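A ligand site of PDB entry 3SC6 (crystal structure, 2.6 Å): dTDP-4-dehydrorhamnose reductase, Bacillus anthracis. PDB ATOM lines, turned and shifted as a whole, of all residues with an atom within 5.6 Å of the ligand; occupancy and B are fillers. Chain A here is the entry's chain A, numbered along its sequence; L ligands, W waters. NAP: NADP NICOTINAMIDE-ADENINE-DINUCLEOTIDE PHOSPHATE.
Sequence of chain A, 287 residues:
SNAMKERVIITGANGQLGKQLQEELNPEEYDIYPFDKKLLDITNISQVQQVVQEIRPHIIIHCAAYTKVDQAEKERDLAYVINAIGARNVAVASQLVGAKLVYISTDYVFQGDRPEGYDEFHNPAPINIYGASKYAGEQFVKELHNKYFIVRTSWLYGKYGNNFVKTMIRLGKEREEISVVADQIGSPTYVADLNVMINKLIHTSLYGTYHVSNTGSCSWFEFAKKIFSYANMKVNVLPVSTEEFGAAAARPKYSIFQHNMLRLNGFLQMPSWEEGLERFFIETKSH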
ATOM      1  N   THR A  11      23.517  -3.612 -28.315  1.00  0.00           N
ATOM      2  CA  THR A  11      22.401  -3.005 -27.595  1.00  0.00           C
ATOM      3  C   THR A  11      22.905  -2.469 -26.256  1.00  0.00           C
ATOM      4  O   THR A  11      23.597  -3.165 -25.529  1.00  0.00           O
ATOM      5  CB  THR A  11      21.253  -4.005 -27.371  1.00  0.00           C
ATOM      6  OG1 THR A  11      21.720  -5.096 -26.561  1.00  0.00           O
ATOM      7  CG2 THR A  11      20.738  -4.542 -28.696  1.00  0.00           C
ATOM      8  N   GLY A  12      22.557  -1.229 -25.928  1.00  0.00           N
ATOM      9  CA  GLY A  12      22.995  -0.604 -24.678  1.00  0.00           C
ATOM     10  C   GLY A  12      24.440  -0.139 -24.843  1.00  0.00           C
ATOM     11  O   GLY A  12      25.278  -0.367 -23.971  1.00  0.00           O
ATOM     12  N   ASN A  14      25.777   2.834 -24.661  1.00  0.00           N
ATOM     13  CA  ASN A  14      26.276   3.887 -23.758  1.00  0.00           C
ATOM     14  C   ASN A  14      26.704   3.388 -22.378  1.00  0.00           C
ATOM     15  O   ASN A  14      27.309   4.145 -21.609  1.00  0.00           O
ATOM     16  CB  ASN A  14      25.255   5.020 -23.600  1.00  0.00           C
ATOM     17  CG  ASN A  14      25.002   5.752 -24.899  1.00  0.00           C
ATOM     18  OD1 ASN A  14      25.562   5.413 -25.937  1.00  0.00           O
ATOM     19  ND2 ASN A  14      24.149   6.776 -24.844  1.00  0.00           N
ATOM     20  N   GLY A  15      26.405   2.134 -22.067  1.00  0.00           N
ATOM     21  CA  GLY A  15      26.770   1.549 -20.768  1.00  0.00           C
ATOM     22  C   GLY A  15      28.246   1.214 -20.673  1.00  0.00           C
ATOM     23  O   GLY A  15      29.007   1.461 -21.610  1.00  0.00           O
ATOM     24  N   GLN A  16      28.643   0.657 -19.548  1.00  0.00           N
ATOM     25  CA  GLN A  16      30.045   0.289 -19.317  1.00  0.00           C
ATOM     26  C   GLN A  16      30.646  -0.566 -20.442  1.00  0.00           C
ATOM     27  O   GLN A  16      31.714  -0.231 -20.951  1.00  0.00           O
ATOM     28  CB  GLN A  16      30.208  -0.438 -17.983  1.00  0.00           C
ATOM     29  CG  GLN A  16      29.820   0.394 -16.773  1.00  0.00           C
ATOM     30  CD  GLN A  16      29.967  -0.355 -15.459  1.00  0.00           C
ATOM     31  OE1 GLN A  16      29.772   0.200 -14.384  1.00  0.00           O
ATOM     32  NE2 GLN A  16      30.324  -1.640 -15.549  1.00  0.00           N
ATOM     33  N   LEU A  17      29.961  -1.653 -20.826  1.00  0.00           N
ATOM     34  CA  LEU A  17      30.468  -2.522 -21.905  1.00  0.00           C
ATOM     35  C   LEU A  17      30.331  -1.909 -23.280  1.00  0.00           C
ATOM     36  O   LEU A  17      31.331  -1.723 -23.972  1.00  0.00           O
ATOM     37  CB  LEU A  17      29.758  -3.878 -21.925  1.00  0.00           C
ATOM     38  CG  LEU A  17      29.973  -4.859 -20.789  1.00  0.00           C
ATOM     39  CD1 LEU A  17      29.163  -6.120 -21.050  1.00  0.00           C
ATOM     40  CD2 LEU A  17      31.450  -5.186 -20.700  1.00  0.00           C
ATOM     41  N   GLY A  18      29.097  -1.642 -23.678  1.00  0.00           N
ATOM     42  CA  GLY A  18      28.811  -1.065 -24.985  1.00  0.00           C
ATOM     43  C   GLY A  18      29.718   0.077 -25.361  1.00  0.00           C
ATOM     44  O   GLY A  18      30.210   0.148 -26.491  1.00  0.00           O
ATOM     45  N   ASP A  36      21.756   3.234 -28.712  1.00  0.00           N
ATOM     46  CA  ASP A  36      21.462   3.669 -27.362  1.00  0.00           C
ATOM     47  C   ASP A  36      20.023   3.260 -27.067  1.00  0.00           C
ATOM     48  O   ASP A  36      19.347   2.659 -27.894  1.00  0.00           O
ATOM     49  CB  ASP A  36      21.627   5.191 -27.247  1.00  0.00           C
ATOM     50  CG  ASP A  36      21.396   5.719 -25.823  1.00  0.00           C
ATOM     51  OD1 ASP A  36      21.288   4.889 -24.890  1.00  0.00           O
ATOM     52  OD2 ASP A  36      21.349   6.961 -25.649  1.00  0.00           O
ATOM     53  N   LYS A  37      19.589   3.588 -25.855  1.00  0.00           N
ATOM     54  CA  LYS A  37      18.243   3.300 -25.377  1.00  0.00           C
ATOM     55  C   LYS A  37      17.154   3.937 -26.264  1.00  0.00           C
ATOM     56  O   LYS A  37      16.149   3.302 -26.560  1.00  0.00           O
ATOM     57  CB  LYS A  37      18.154   3.824 -23.936  1.00  0.00           C
ATOM     58  CG  LYS A  37      16.855   3.618 -23.197  1.00  0.00           C
ATOM     59  CD  LYS A  37      16.977   4.225 -21.805  1.00  0.00           C
ATOM     60  CE  LYS A  37      15.712   4.074 -20.986  1.00  0.00           C
ATOM     61  NZ  LYS A  37      15.877   4.697 -19.633  1.00  0.00           N
ATOM     62  N   LEU A  40      17.231   2.358 -30.010  1.00  0.00           N
ATOM     63  CA  LEU A  40      16.846   0.942 -30.023  1.00  0.00           C
ATOM     64  C   LEU A  40      16.328   0.522 -28.658  1.00  0.00           C
ATOM     65  O   LEU A  40      17.080   0.035 -27.807  1.00  0.00           O
ATOM     66  CB  LEU A  40      18.035   0.055 -30.424  1.00  0.00           C
ATOM     67  CG  LEU A  40      17.792  -1.458 -30.472  1.00  0.00           C
ATOM     68  CD1 LEU A  40      16.634  -1.810 -31.395  1.00  0.00           C
ATOM     69  CD2 LEU A  40      19.062  -2.201 -30.901  1.00  0.00           C
ATOM     70  N   ASP A  41      15.031   0.741 -28.442  1.00  0.00           N
ATOM     71  CA  ASP A  41      14.393   0.393 -27.171  1.00  0.00           C
ATOM     72  C   ASP A  41      14.132  -1.116 -27.161  1.00  0.00           C
ATOM     73  O   ASP A  41      13.295  -1.620 -27.903  1.00  0.00           O
ATOM     74  CB  ASP A  41      13.094   1.179 -26.986  1.00  0.00           C
ATOM     75  CG  ASP A  41      12.427   0.882 -25.660  1.00  0.00           C
ATOM     76  OD1 ASP A  41      12.936   0.040 -24.899  1.00  0.00           O
ATOM     77  OD2 ASP A  41      11.381   1.500 -25.380  1.00  0.00           O
ATOM     78  N   ILE A  42      14.870  -1.810 -26.302  1.00  0.00           N
ATOM     79  CA  ILE A  42      14.769  -3.258 -26.165  1.00  0.00           C
ATOM     80  C   ILE A  42      13.341  -3.718 -25.853  1.00  0.00           C
ATOM     81  O   ILE A  42      12.923  -4.793 -26.287  1.00  0.00           O
ATOM     82  CB  ILE A  42      15.698  -3.724 -25.014  1.00  0.00           C
ATOM     83  CG1 ILE A  42      15.867  -5.234 -24.988  1.00  0.00           C
ATOM     84  CG2 ILE A  42      15.192  -3.223 -23.682  1.00  0.00           C
ATOM     85  CD1 ILE A  42      16.749  -5.684 -23.828  1.00  0.00           C
ATOM     86  N   THR A  43      12.588  -2.897 -25.118  1.00  0.00           N
ATOM     87  CA  THR A  43      11.208  -3.234 -24.746  1.00  0.00           C
ATOM     88  C   THR A  43      10.186  -3.017 -25.864  1.00  0.00           C
ATOM     89  O   THR A  43       9.008  -3.335 -25.688  1.00  0.00           O
ATOM     90  CB  THR A  43      10.752  -2.436 -23.516  1.00  0.00           C
ATOM     91  OG1 THR A  43      10.766  -1.034 -23.812  1.00  0.00           O
ATOM     92  CG2 THR A  43      11.671  -2.713 -22.335  1.00  0.00           C
ATOM     93  N   HIS A  62      24.242  -8.347 -27.060  1.00  0.00           N
ATOM     94  CA  HIS A  62      23.218  -7.755 -26.240  1.00  0.00           C
ATOM     95  C   HIS A  62      23.733  -7.319 -24.866  1.00  0.00           C
ATOM     96  O   HIS A  62      23.891  -8.148 -23.964  1.00  0.00           O
ATOM     97  CB  HIS A  62      22.086  -8.764 -26.083  1.00  0.00           C
ATOM     98  CG  HIS A  62      20.895  -8.220 -25.372  1.00  0.00           C
ATOM     99  ND1 HIS A  62      19.865  -7.581 -26.047  1.00  0.00           N
ATOM    100  CD2 HIS A  62      20.534  -8.234 -24.074  1.00  0.00           C
ATOM    101  CE1 HIS A  62      18.937  -7.216 -25.178  1.00  0.00           C
ATOM    102  NE2 HIS A  62      19.321  -7.603 -23.975  1.00  0.00           N
ATOM    103  N   CYS A  63      23.973  -6.026 -24.710  1.00  0.00           N
ATOM    104  CA  CYS A  63      24.468  -5.476 -23.448  1.00  0.00           C
ATOM    105  C   CYS A  63      23.374  -4.722 -22.678  1.00  0.00           C
ATOM    106  O   CYS A  63      23.523  -4.491 -21.477  1.00  0.00           O
ATOM    107  CB  CYS A  63      25.643  -4.535 -23.700  1.00  0.00           C
ATOM    108  SG  CYS A  63      27.043  -5.332 -24.540  1.00  0.00           S
ATOM    109  N   ALA A  64      22.296  -4.354 -23.360  1.00  0.00           N
ATOM    110  CA  ALA A  64      21.190  -3.638 -22.730  1.00  0.00           C
ATOM    111  C   ALA A  64      20.659  -4.385 -21.509  1.00  0.00           C
ATOM    112  O   ALA A  64      20.508  -5.617 -21.539  1.00  0.00           O
ATOM    113  CB  ALA A  64      20.063  -3.402 -23.736  1.00  0.00           C
ATOM    114  N   ALA A  65      20.391  -3.645 -20.427  1.00  0.00           N
ATOM    115  CA  ALA A  65      19.881  -4.249 -19.201  1.00  0.00           C
ATOM    116  C   ALA A  65      19.634  -3.222 -18.093  1.00  0.00           C
ATOM    117  O   ALA A  65      20.149  -2.099 -18.126  1.00  0.00           O
ATOM    118  CB  ALA A  65      20.847  -5.308 -18.701  1.00  0.00           C
ATOM    119  N   TYR A  66      18.831  -3.626 -17.116  1.00  0.00           N
ATOM    120  CA  TYR A  66      18.480  -2.808 -15.973  1.00  0.00           C
ATOM    121  C   TYR A  66      19.417  -3.317 -14.891  1.00  0.00           C
ATOM    122  O   TYR A  66      19.148  -4.337 -14.254  1.00  0.00           O
ATOM    123  CB  TYR A  66      17.012  -3.032 -15.584  1.00  0.00           C
ATOM    124  CG  TYR A  66      16.537  -2.217 -14.408  1.00  0.00           C
ATOM    125  CD1 TYR A  66      15.994  -0.949 -14.594  1.00  0.00           C
ATOM    126  CD2 TYR A  66      16.615  -2.715 -13.115  1.00  0.00           C
ATOM    127  CE1 TYR A  66      15.544  -0.198 -13.513  1.00  0.00           C
ATOM    128  CE2 TYR A  66      16.174  -1.966 -12.034  1.00  0.00           C
ATOM    129  CZ  TYR A  66      15.637  -0.715 -12.246  1.00  0.00           C
ATOM    130  OH  TYR A  66      15.207   0.032 -11.166  1.00  0.00           O
ATOM    131  N   THR A  67      20.527  -2.607 -14.691  1.00  0.00           N
ATOM    132  CA  THR A  67      21.538  -2.999 -13.703  1.00  0.00           C
ATOM    133  C   THR A  67      21.457  -2.283 -12.354  1.00  0.00           C
ATOM    134  O   THR A  67      22.489  -2.001 -11.734  1.00  0.00           O
ATOM    135  CB  THR A  67      22.941  -2.767 -14.274  1.00  0.00           C
ATOM    136  OG1 THR A  67      23.131  -1.362 -14.528  1.00  0.00           O
ATOM    137  CG2 THR A  67      23.122  -3.549 -15.564  1.00  0.00           C
ATOM    138  N   ILE A  82      12.642  -5.182 -18.908  1.00  0.00           N
ATOM    139  CA  ILE A  82      13.925  -4.922 -19.548  1.00  0.00           C
ATOM    140  C   ILE A  82      14.790  -6.166 -19.720  1.00  0.00           C
ATOM    141  O   ILE A  82      15.153  -6.503 -20.834  1.00  0.00           O
ATOM    142  CB  ILE A  82      14.765  -3.887 -18.758  1.00  0.00           C
ATOM    143  CG1 ILE A  82      14.042  -2.543 -18.668  1.00  0.00           C
ATOM    144  CG2 ILE A  82      16.120  -3.669 -19.443  1.00  0.00           C
ATOM    145  CD1 ILE A  82      13.766  -1.919 -19.993  1.00  0.00           C
ATOM    146  N   ASN A  83      15.125  -6.817 -18.612  1.00  0.00           N
ATOM    147  CA  ASN A  83      15.974  -8.012 -18.635  1.00  0.00           C
ATOM    148  C   ASN A  83      15.394  -9.296 -19.224  1.00  0.00           C
ATOM    149  O   ASN A  83      16.106 -10.030 -19.910  1.00  0.00           O
ATOM    150  CB  ASN A  83      16.509  -8.298 -17.223  1.00  0.00           C
ATOM    151  CG  ASN A  83      17.454  -7.209 -16.717  1.00  0.00           C
ATOM    152  OD1 ASN A  83      17.891  -6.345 -17.475  1.00  0.00           O
ATOM    153  ND2 ASN A  83      17.815  -7.287 -15.448  1.00  0.00           N
ATOM    154  N   ILE A 104      24.818 -11.186 -22.282  1.00  0.00           N
ATOM    155  CA  ILE A 104      25.625 -10.984 -21.098  1.00  0.00           C
ATOM    156  C   ILE A 104      24.761 -11.183 -19.868  1.00  0.00           C
ATOM    157  O   ILE A 104      23.728 -10.538 -19.712  1.00  0.00           O
ATOM    158  CB  ILE A 104      26.243  -9.580 -21.068  1.00  0.00           C
ATOM    159  CG1 ILE A 104      27.112  -9.355 -22.313  1.00  0.00           C
ATOM    160  CG2 ILE A 104      27.098  -9.402 -19.829  1.00  0.00           C
ATOM    161  CD1 ILE A 104      28.260 -10.330 -22.444  1.00  0.00           C
ATOM    162  N   SER A 105      25.187 -12.095 -18.995  1.00  0.00           N
ATOM    163  CA  SER A 105      24.447 -12.385 -17.778  1.00  0.00           C
ATOM    164  C   SER A 105      25.293 -12.155 -16.534  1.00  0.00           C
ATOM    165  O   SER A 105      26.419 -11.661 -16.618  1.00  0.00           O
ATOM    166  CB  SER A 105      23.896 -13.809 -17.818  1.00  0.00           C
ATOM    167  OG  SER A 105      23.136 -14.091 -16.650  1.00  0.00           O
ATOM    168  N   THR A 106      24.747 -12.533 -15.378  1.00  0.00           N
ATOM    169  CA  THR A 106      25.420 -12.349 -14.091  1.00  0.00           C
ATOM    170  C   THR A 106      25.526 -13.565 -13.173  1.00  0.00           C
ATOM    171  O   THR A 106      24.935 -14.615 -13.430  1.00  0.00           O
ATOM    172  CB  THR A 106      24.615 -11.301 -13.295  1.00  0.00           C
ATOM    173  OG1 THR A 106      25.247 -11.065 -12.032  1.00  0.00           O
ATOM    174  CG2 THR A 106      23.187 -11.792 -13.070  1.00  0.00           C
ATOM    175  N   ASP A 107      26.290 -13.402 -12.100  1.00  0.00           N
ATOM    176  CA  ASP A 107      26.482 -14.465 -11.123  1.00  0.00           C
ATOM    177  C   ASP A 107      25.358 -14.470 -10.085  1.00  0.00           C
ATOM    178  O   ASP A 107      25.310 -15.347  -9.227  1.00  0.00           O
ATOM    179  CB  ASP A 107      27.845 -14.323 -10.414  1.00  0.00           C
ATOM    180  CG  ASP A 107      27.999 -12.989  -9.705  1.00  0.00           C
ATOM    181  OD1 ASP A 107      28.555 -12.989  -8.595  1.00  0.00           O
ATOM    182  OD2 ASP A 107      27.589 -11.952 -10.256  1.00  0.00           O
ATOM    183  N   TYR A 108      24.459 -13.494 -10.159  1.00  0.00           N
ATOM    184  CA  TYR A 108      23.339 -13.417  -9.217  1.00  0.00           C
ATOM    185  C   TYR A 108      22.243 -14.423  -9.561  1.00  0.00           C
ATOM    186  O   TYR A 108      21.170 -14.410  -8.976  1.00  0.00           O
ATOM    187  CB  TYR A 108      22.756 -11.998  -9.099  1.00  0.00           C
ATOM    188  CG  TYR A 108      23.717 -10.984  -8.516  1.00  0.00           C
ATOM    189  CD1 TYR A 108      24.136 -11.088  -7.194  1.00  0.00           C
ATOM    190  CD2 TYR A 108      24.161  -9.904  -9.251  1.00  0.00           C
ATOM    191  CE1 TYR A 108      25.005 -10.163  -6.648  1.00  0.00           C
ATOM    192  CE2 TYR A 108      25.032  -8.971  -8.711  1.00  0.00           C
ATOM    193  CZ  TYR A 108      25.443  -9.106  -7.404  1.00  0.00           C
ATOM    194  OH  TYR A 108      26.304  -8.174  -6.850  1.00  0.00           O
ATOM    195  N   TYR A 130      17.187  -8.941  -9.494  1.00  0.00           N
ATOM    196  CA  TYR A 130      18.065  -8.733 -10.648  1.00  0.00           C
ATOM    197  C   TYR A 130      18.497 -10.073 -11.224  1.00  0.00           C
ATOM    198  O   TYR A 130      18.368 -10.309 -12.425  1.00  0.00           O
ATOM    199  CB  TYR A 130      19.285  -7.915 -10.260  1.00  0.00           C
ATOM    200  CG  TYR A 130      20.366  -7.828 -11.316  1.00  0.00           C
ATOM    201  CD1 TYR A 130      20.304  -6.912 -12.355  1.00  0.00           C
ATOM    202  CD2 TYR A 130      21.493  -8.642 -11.234  1.00  0.00           C
ATOM    203  CE1 TYR A 130      21.313  -6.834 -13.313  1.00  0.00           C
ATOM    204  CE2 TYR A 130      22.501  -8.576 -12.173  1.00  0.00           C
ATOM    205  CZ  TYR A 130      22.407  -7.670 -13.201  1.00  0.00           C
ATOM    206  OH  TYR A 130      23.432  -7.620 -14.121  1.00  0.00           O
ATOM    207  N   LYS A 134      17.351 -11.710 -15.059  1.00  0.00           N
ATOM    208  CA  LYS A 134      18.213 -12.114 -16.164  1.00  0.00           C
ATOM    209  C   LYS A 134      18.201 -13.619 -16.395  1.00  0.00           C
ATOM    210  O   LYS A 134      18.449 -14.064 -17.509  1.00  0.00           O
ATOM    211  CB  LYS A 134      19.628 -11.532 -16.112  1.00  0.00           C
ATOM    212  CG  LYS A 134      19.595 -10.008 -16.132  1.00  0.00           C
ATOM    213  CD  LYS A 134      20.934  -9.389 -16.466  1.00  0.00           C
ATOM    214  CE  LYS A 134      21.304  -9.743 -17.911  1.00  0.00           C
ATOM    215  NZ  LYS A 134      22.581  -9.156 -18.392  1.00  0.00           N
ATOM    216  N   THR A 153      29.136 -12.884 -16.240  1.00  0.00           N
ATOM    217  CA  THR A 153      30.308 -12.214 -15.720  1.00  0.00           C
ATOM    218  C   THR A 153      29.947 -11.666 -14.345  1.00  0.00           C
ATOM    219  O   THR A 153      28.829 -11.889 -13.883  1.00  0.00           O
ATOM    220  CB  THR A 153      30.769 -11.071 -16.637  1.00  0.00           C
ATOM    221  OG1 THR A 153      32.021 -10.550 -16.159  1.00  0.00           O
ATOM    222  CG2 THR A 153      29.713  -9.973 -16.699  1.00  0.00           C
ATOM    223  N   SER A 154      30.867 -10.949 -13.696  1.00  0.00           N
ATOM    224  CA  SER A 154      30.597 -10.397 -12.361  1.00  0.00           C
ATOM    225  C   SER A 154      31.597  -9.326 -11.923  1.00  0.00           C
ATOM    226  O   SER A 154      32.754  -9.357 -12.358  1.00  0.00           O
ATOM    227  CB  SER A 154      30.666 -11.522 -11.328  1.00  0.00           C
ATOM    228  OG  SER A 154      31.951 -12.114 -11.321  1.00  0.00           O
ATOM    229  N   TRP A 155      31.158  -8.396 -11.068  1.00  0.00           N
ATOM    230  CA  TRP A 155      32.063  -7.342 -10.593  1.00  0.00           C
ATOM    231  C   TRP A 155      32.766  -6.705 -11.764  1.00  0.00           C
ATOM    232  O   TRP A 155      33.988  -6.541 -11.773  1.00  0.00           O
ATOM    233  CB  TRP A 155      33.048  -8.000  -9.619  1.00  0.00           C
ATOM    234  CG  TRP A 155      32.416  -8.416  -8.320  1.00  0.00           C
ATOM    235  CD1 TRP A 155      31.291  -9.160  -8.158  1.00  0.00           C
ATOM    236  CD2 TRP A 155      33.034  -8.349  -7.026  1.00  0.00           C
ATOM    237  NE1 TRP A 155      31.073  -9.417  -6.820  1.00  0.00           N
ATOM    238  CE2 TRP A 155      32.145  -8.956  -6.113  1.00  0.00           C
ATOM    239  CE3 TRP A 155      34.222  -7.791  -6.548  1.00  0.00           C
ATOM    240  CZ2 TRP A 155      32.411  -9.014  -4.747  1.00  0.00           C
ATOM    241  CZ3 TRP A 155      34.486  -7.854  -5.191  1.00  0.00           C
ATOM    242  CH2 TRP A 155      33.587  -8.458  -4.314  1.00  0.00           C
ATOM    243  N   LEU A 156      31.972  -6.351 -12.765  1.00  0.00           N
ATOM    244  CA  LEU A 156      32.464  -5.737 -13.982  1.00  0.00           C
ATOM    245  C   LEU A 156      32.738  -4.242 -13.799  1.00  0.00           C
ATOM    246  O   LEU A 156      31.965  -3.553 -13.147  1.00  0.00           O
ATOM    247  CB  LEU A 156      31.420  -5.959 -15.082  1.00  0.00           C
ATOM    248  CG  LEU A 156      31.727  -5.514 -16.511  1.00  0.00           C
ATOM    249  CD1 LEU A 156      32.956  -6.241 -17.024  1.00  0.00           C
ATOM    250  CD2 LEU A 156      30.531  -5.808 -17.391  1.00  0.00           C
HETATM  251  PA  NAP L   1      25.095  -0.479 -17.630  1.00  0.00           P
HETATM  252  O1A NAP L   1      23.876  -0.175 -16.796  1.00  0.00           O
HETATM  253  O2A NAP L   1      26.157   0.590 -17.788  1.00  0.00           O
HETATM  254  O5B NAP L   1      24.633  -0.940 -19.103  1.00  0.00           O
HETATM  255  C5B NAP L   1      23.266  -1.210 -19.406  1.00  0.00           C
HETATM  256  C4B NAP L   1      22.804  -0.246 -20.493  1.00  0.00           C
HETATM  257  O4B NAP L   1      21.515  -0.651 -20.987  1.00  0.00           O
HETATM  258  C3B NAP L   1      22.656   1.182 -19.956  1.00  0.00           C
HETATM  259  O3B NAP L   1      23.444   2.109 -20.714  1.00  0.00           O
HETATM  260  C2B NAP L   1      21.183   1.493 -20.108  1.00  0.00           C
HETATM  261  O2B NAP L   1      20.962   2.857 -20.461  1.00  0.00           O
HETATM  262  C1B NAP L   1      20.747   0.527 -21.214  1.00  0.00           C
HETATM  263  N9A NAP L   1      19.274   0.340 -21.245  1.00  0.00           N
HETATM  264  C8A NAP L   1      18.404   0.477 -20.226  1.00  0.00           C
HETATM  265  N7A NAP L   1      17.152   0.241 -20.686  1.00  0.00           N
HETATM  266  C5A NAP L   1      17.256  -0.040 -22.002  1.00  0.00           C
HETATM  267  C6A NAP L   1      16.281  -0.375 -23.070  1.00  0.00           C
HETATM  268  N6A NAP L   1      14.953  -0.455 -22.788  1.00  0.00           N
HETATM  269  N1A NAP L   1      16.744  -0.611 -24.318  1.00  0.00           N
HETATM  270  C2A NAP L   1      18.065  -0.519 -24.582  1.00  0.00           C
HETATM  271  N3A NAP L   1      18.968  -0.216 -23.625  1.00  0.00           N
HETATM  272  C4A NAP L   1      18.589   0.024 -22.346  1.00  0.00           C
HETATM  273  O3  NAP L   1      25.786  -1.827 -17.067  1.00  0.00           O
HETATM  274  PN  NAP L   1      26.877  -2.678 -17.897  1.00  0.00           P
HETATM  275  O1N NAP L   1      27.841  -3.292 -16.898  1.00  0.00           O
HETATM  276  O2N NAP L   1      27.404  -1.864 -19.051  1.00  0.00           O
HETATM  277  O5D NAP L   1      26.000  -3.865 -18.520  1.00  0.00           O
HETATM  278  C5D NAP L   1      26.624  -4.971 -19.159  1.00  0.00           C
HETATM  279  C4D NAP L   1      25.885  -6.272 -18.832  1.00  0.00           C
HETATM  280  O4D NAP L   1      26.614  -7.023 -17.856  1.00  0.00           O
HETATM  281  C3D NAP L   1      24.491  -6.034 -18.272  1.00  0.00           C
HETATM  282  O3D NAP L   1      23.524  -6.756 -19.040  1.00  0.00           O
HETATM  283  C2D NAP L   1      24.534  -6.563 -16.849  1.00  0.00           C
HETATM  284  O2D NAP L   1      23.309  -7.221 -16.522  1.00  0.00           O
HETATM  285  C1D NAP L   1      25.724  -7.506 -16.841  1.00  0.00           C
HETATM  286  N1N NAP L   1      26.412  -7.590 -15.538  1.00  0.00           N
HETATM  287  C2N NAP L   1      26.952  -6.486 -15.000  1.00  0.00           C
HETATM  288  C3N NAP L   1      27.602  -6.546 -13.765  1.00  0.00           C
HETATM  289  C7N NAP L   1      28.195  -5.293 -13.182  1.00  0.00           C
HETATM  290  O7N NAP L   1      28.024  -4.235 -13.761  1.00  0.00           O
HETATM  291  N7N NAP L   1      28.893  -5.353 -12.048  1.00  0.00           N
HETATM  292  C4N NAP L   1      27.698  -7.769 -13.111  1.00  0.00           C
HETATM  293  C5N NAP L   1      27.142  -8.897 -13.692  1.00  0.00           C
HETATM  294  C6N NAP L   1      26.495  -8.778 -14.927  1.00  0.00           C
HETATM  295  P2B NAP L   1      20.380   3.898 -19.378  1.00  0.00           P
HETATM  296  O1X NAP L   1      20.552   5.232 -20.058  1.00  0.00           O
HETATM  297  O2X NAP L   1      18.938   3.490 -19.178  1.00  0.00           O
HETATM  298  O3X NAP L   1      21.256   3.702 -18.157  1.00  0.00           O
HETATM  299  O   HOH W   1      22.593   2.615 -23.898  1.00  0.00           O
HETATM  300  O   HOH W   2      26.693  -1.660 -21.584  1.00  0.00           O
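Water W2 lies within hydrogen-bond range of an oxygen (O2N) of the ligand (2.6 Å), the backbone carbonyl oxygen of Gly 12 (3.1 Å), the backbone NH of Gly 18 (3.2 Å) and the backbone NH of Leu 17 (3.4 Å). Water W1 lies within hydrogen-bond range of OD1 of Asp 36, N of Asn 14 and O3B of the ligand.
OG1 of Thr 106 sits at hydrogen-bond distance from N of Tyr 108 (3.2 Å). O of Leu 156 is in hydrogen-bond range of NE2 of Gln 16 (3.5 Å). A ring nitrogen (NE2) of His 62 lies within hydrogen-bond range of the backbone carbonyl oxygen (O) of Ala 64, 3.4 Å away. The backbone carbonyl oxygen of Ser 105 is in hydrogen-bond range of the backbone NH of Thr 153, at 3.0 Å. OD1 of Asp 41 sits at hydrogen-bond distance from OG1 of Thr 43 (2.7 Å). The side-chain hydroxyl of Thr 106 lies within hydrogen-bond range of the side-chain carboxylate of Asp 107. ND2 of Asn 14 lies within hydrogen-bond range of OD2 of Asp 36 (2.9 Å). The backbone NH (N) of Cys 63 lies within hydrogen-bond range of the backbone carbonyl oxygen (O) of Thr 11, 3.0 Å away.
N7N of the ligand sits close to N of Leu 156, at 3.3 Å. Residues that only touch the ligand: Gly 12 (3.98 Å), Asn 14 (3.9 Å), Leu 40 (3.4 Å), Ala 64 (3.4 Å), Ile 82 (3.4 Å), Ile 104 (3.1 Å), Ser 105 (3.3 Å), Thr 106 (3.3 Å), Thr 153 (3.4 Å), Ser 154 (3.98 Å) and Trp 155 (3.9 Å). 23 residues have an atom within 4 Å of the ligand: Gly 12, Asn 14, Gly 15, Gln 16, Leu 17, Lys 37, Leu 40, Asp 41, Ile 42, Cys 63, Ala 64, Ala 65, Thr 67, Ile 82, Ile 104, Ser 105, Thr 106, Tyr 130, Lys 134, Thr 153, Ser 154, Trp 155 and Leu 156.
An oxygen (O2N) of the ligand is in hydrogen-bond range of the backbone NH (N) of Gln 16, at 2.9 Å. An oxygen (O3D) of the ligand sits at hydrogen-bond distance from the side-chain amino group of Lys 134, 2.7 Å away. N of Ile 42 is in hydrogen-bond range of N1A of the ligand (3.0 Å). O3D of the ligand sits at hydrogen-bond distance from O of Cys 63 (3.3 Å). O1N of the ligand lies within hydrogen-bond range of NE2 of Gln 16. O2X of the ligand lies within salt-bridge range of NZ of Lys 37 (3.3 Å). A nitrogen (N6A) of the ligand is in hydrogen-bond range of the side-chain carboxylate (OD1) of Asp 41, 3.0 Å away. The side-chain hydroxyl of Thr 67 is in hydrogen-bond range of an oxygen (O1A) of the ligand. O2D of the ligand is in hydrogen-bond range of OH of Tyr 130 (2.4 Å). O4B of the ligand is in hydrogen-bond range of N of Ala 65 (3.2 Å). O2N of the ligand is in hydrogen-bond range of N of Leu 17 (3.1 Å). N of Gly 15 sits at hydrogen-bond distance from O3B of the ligand, 3.3 Å away.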
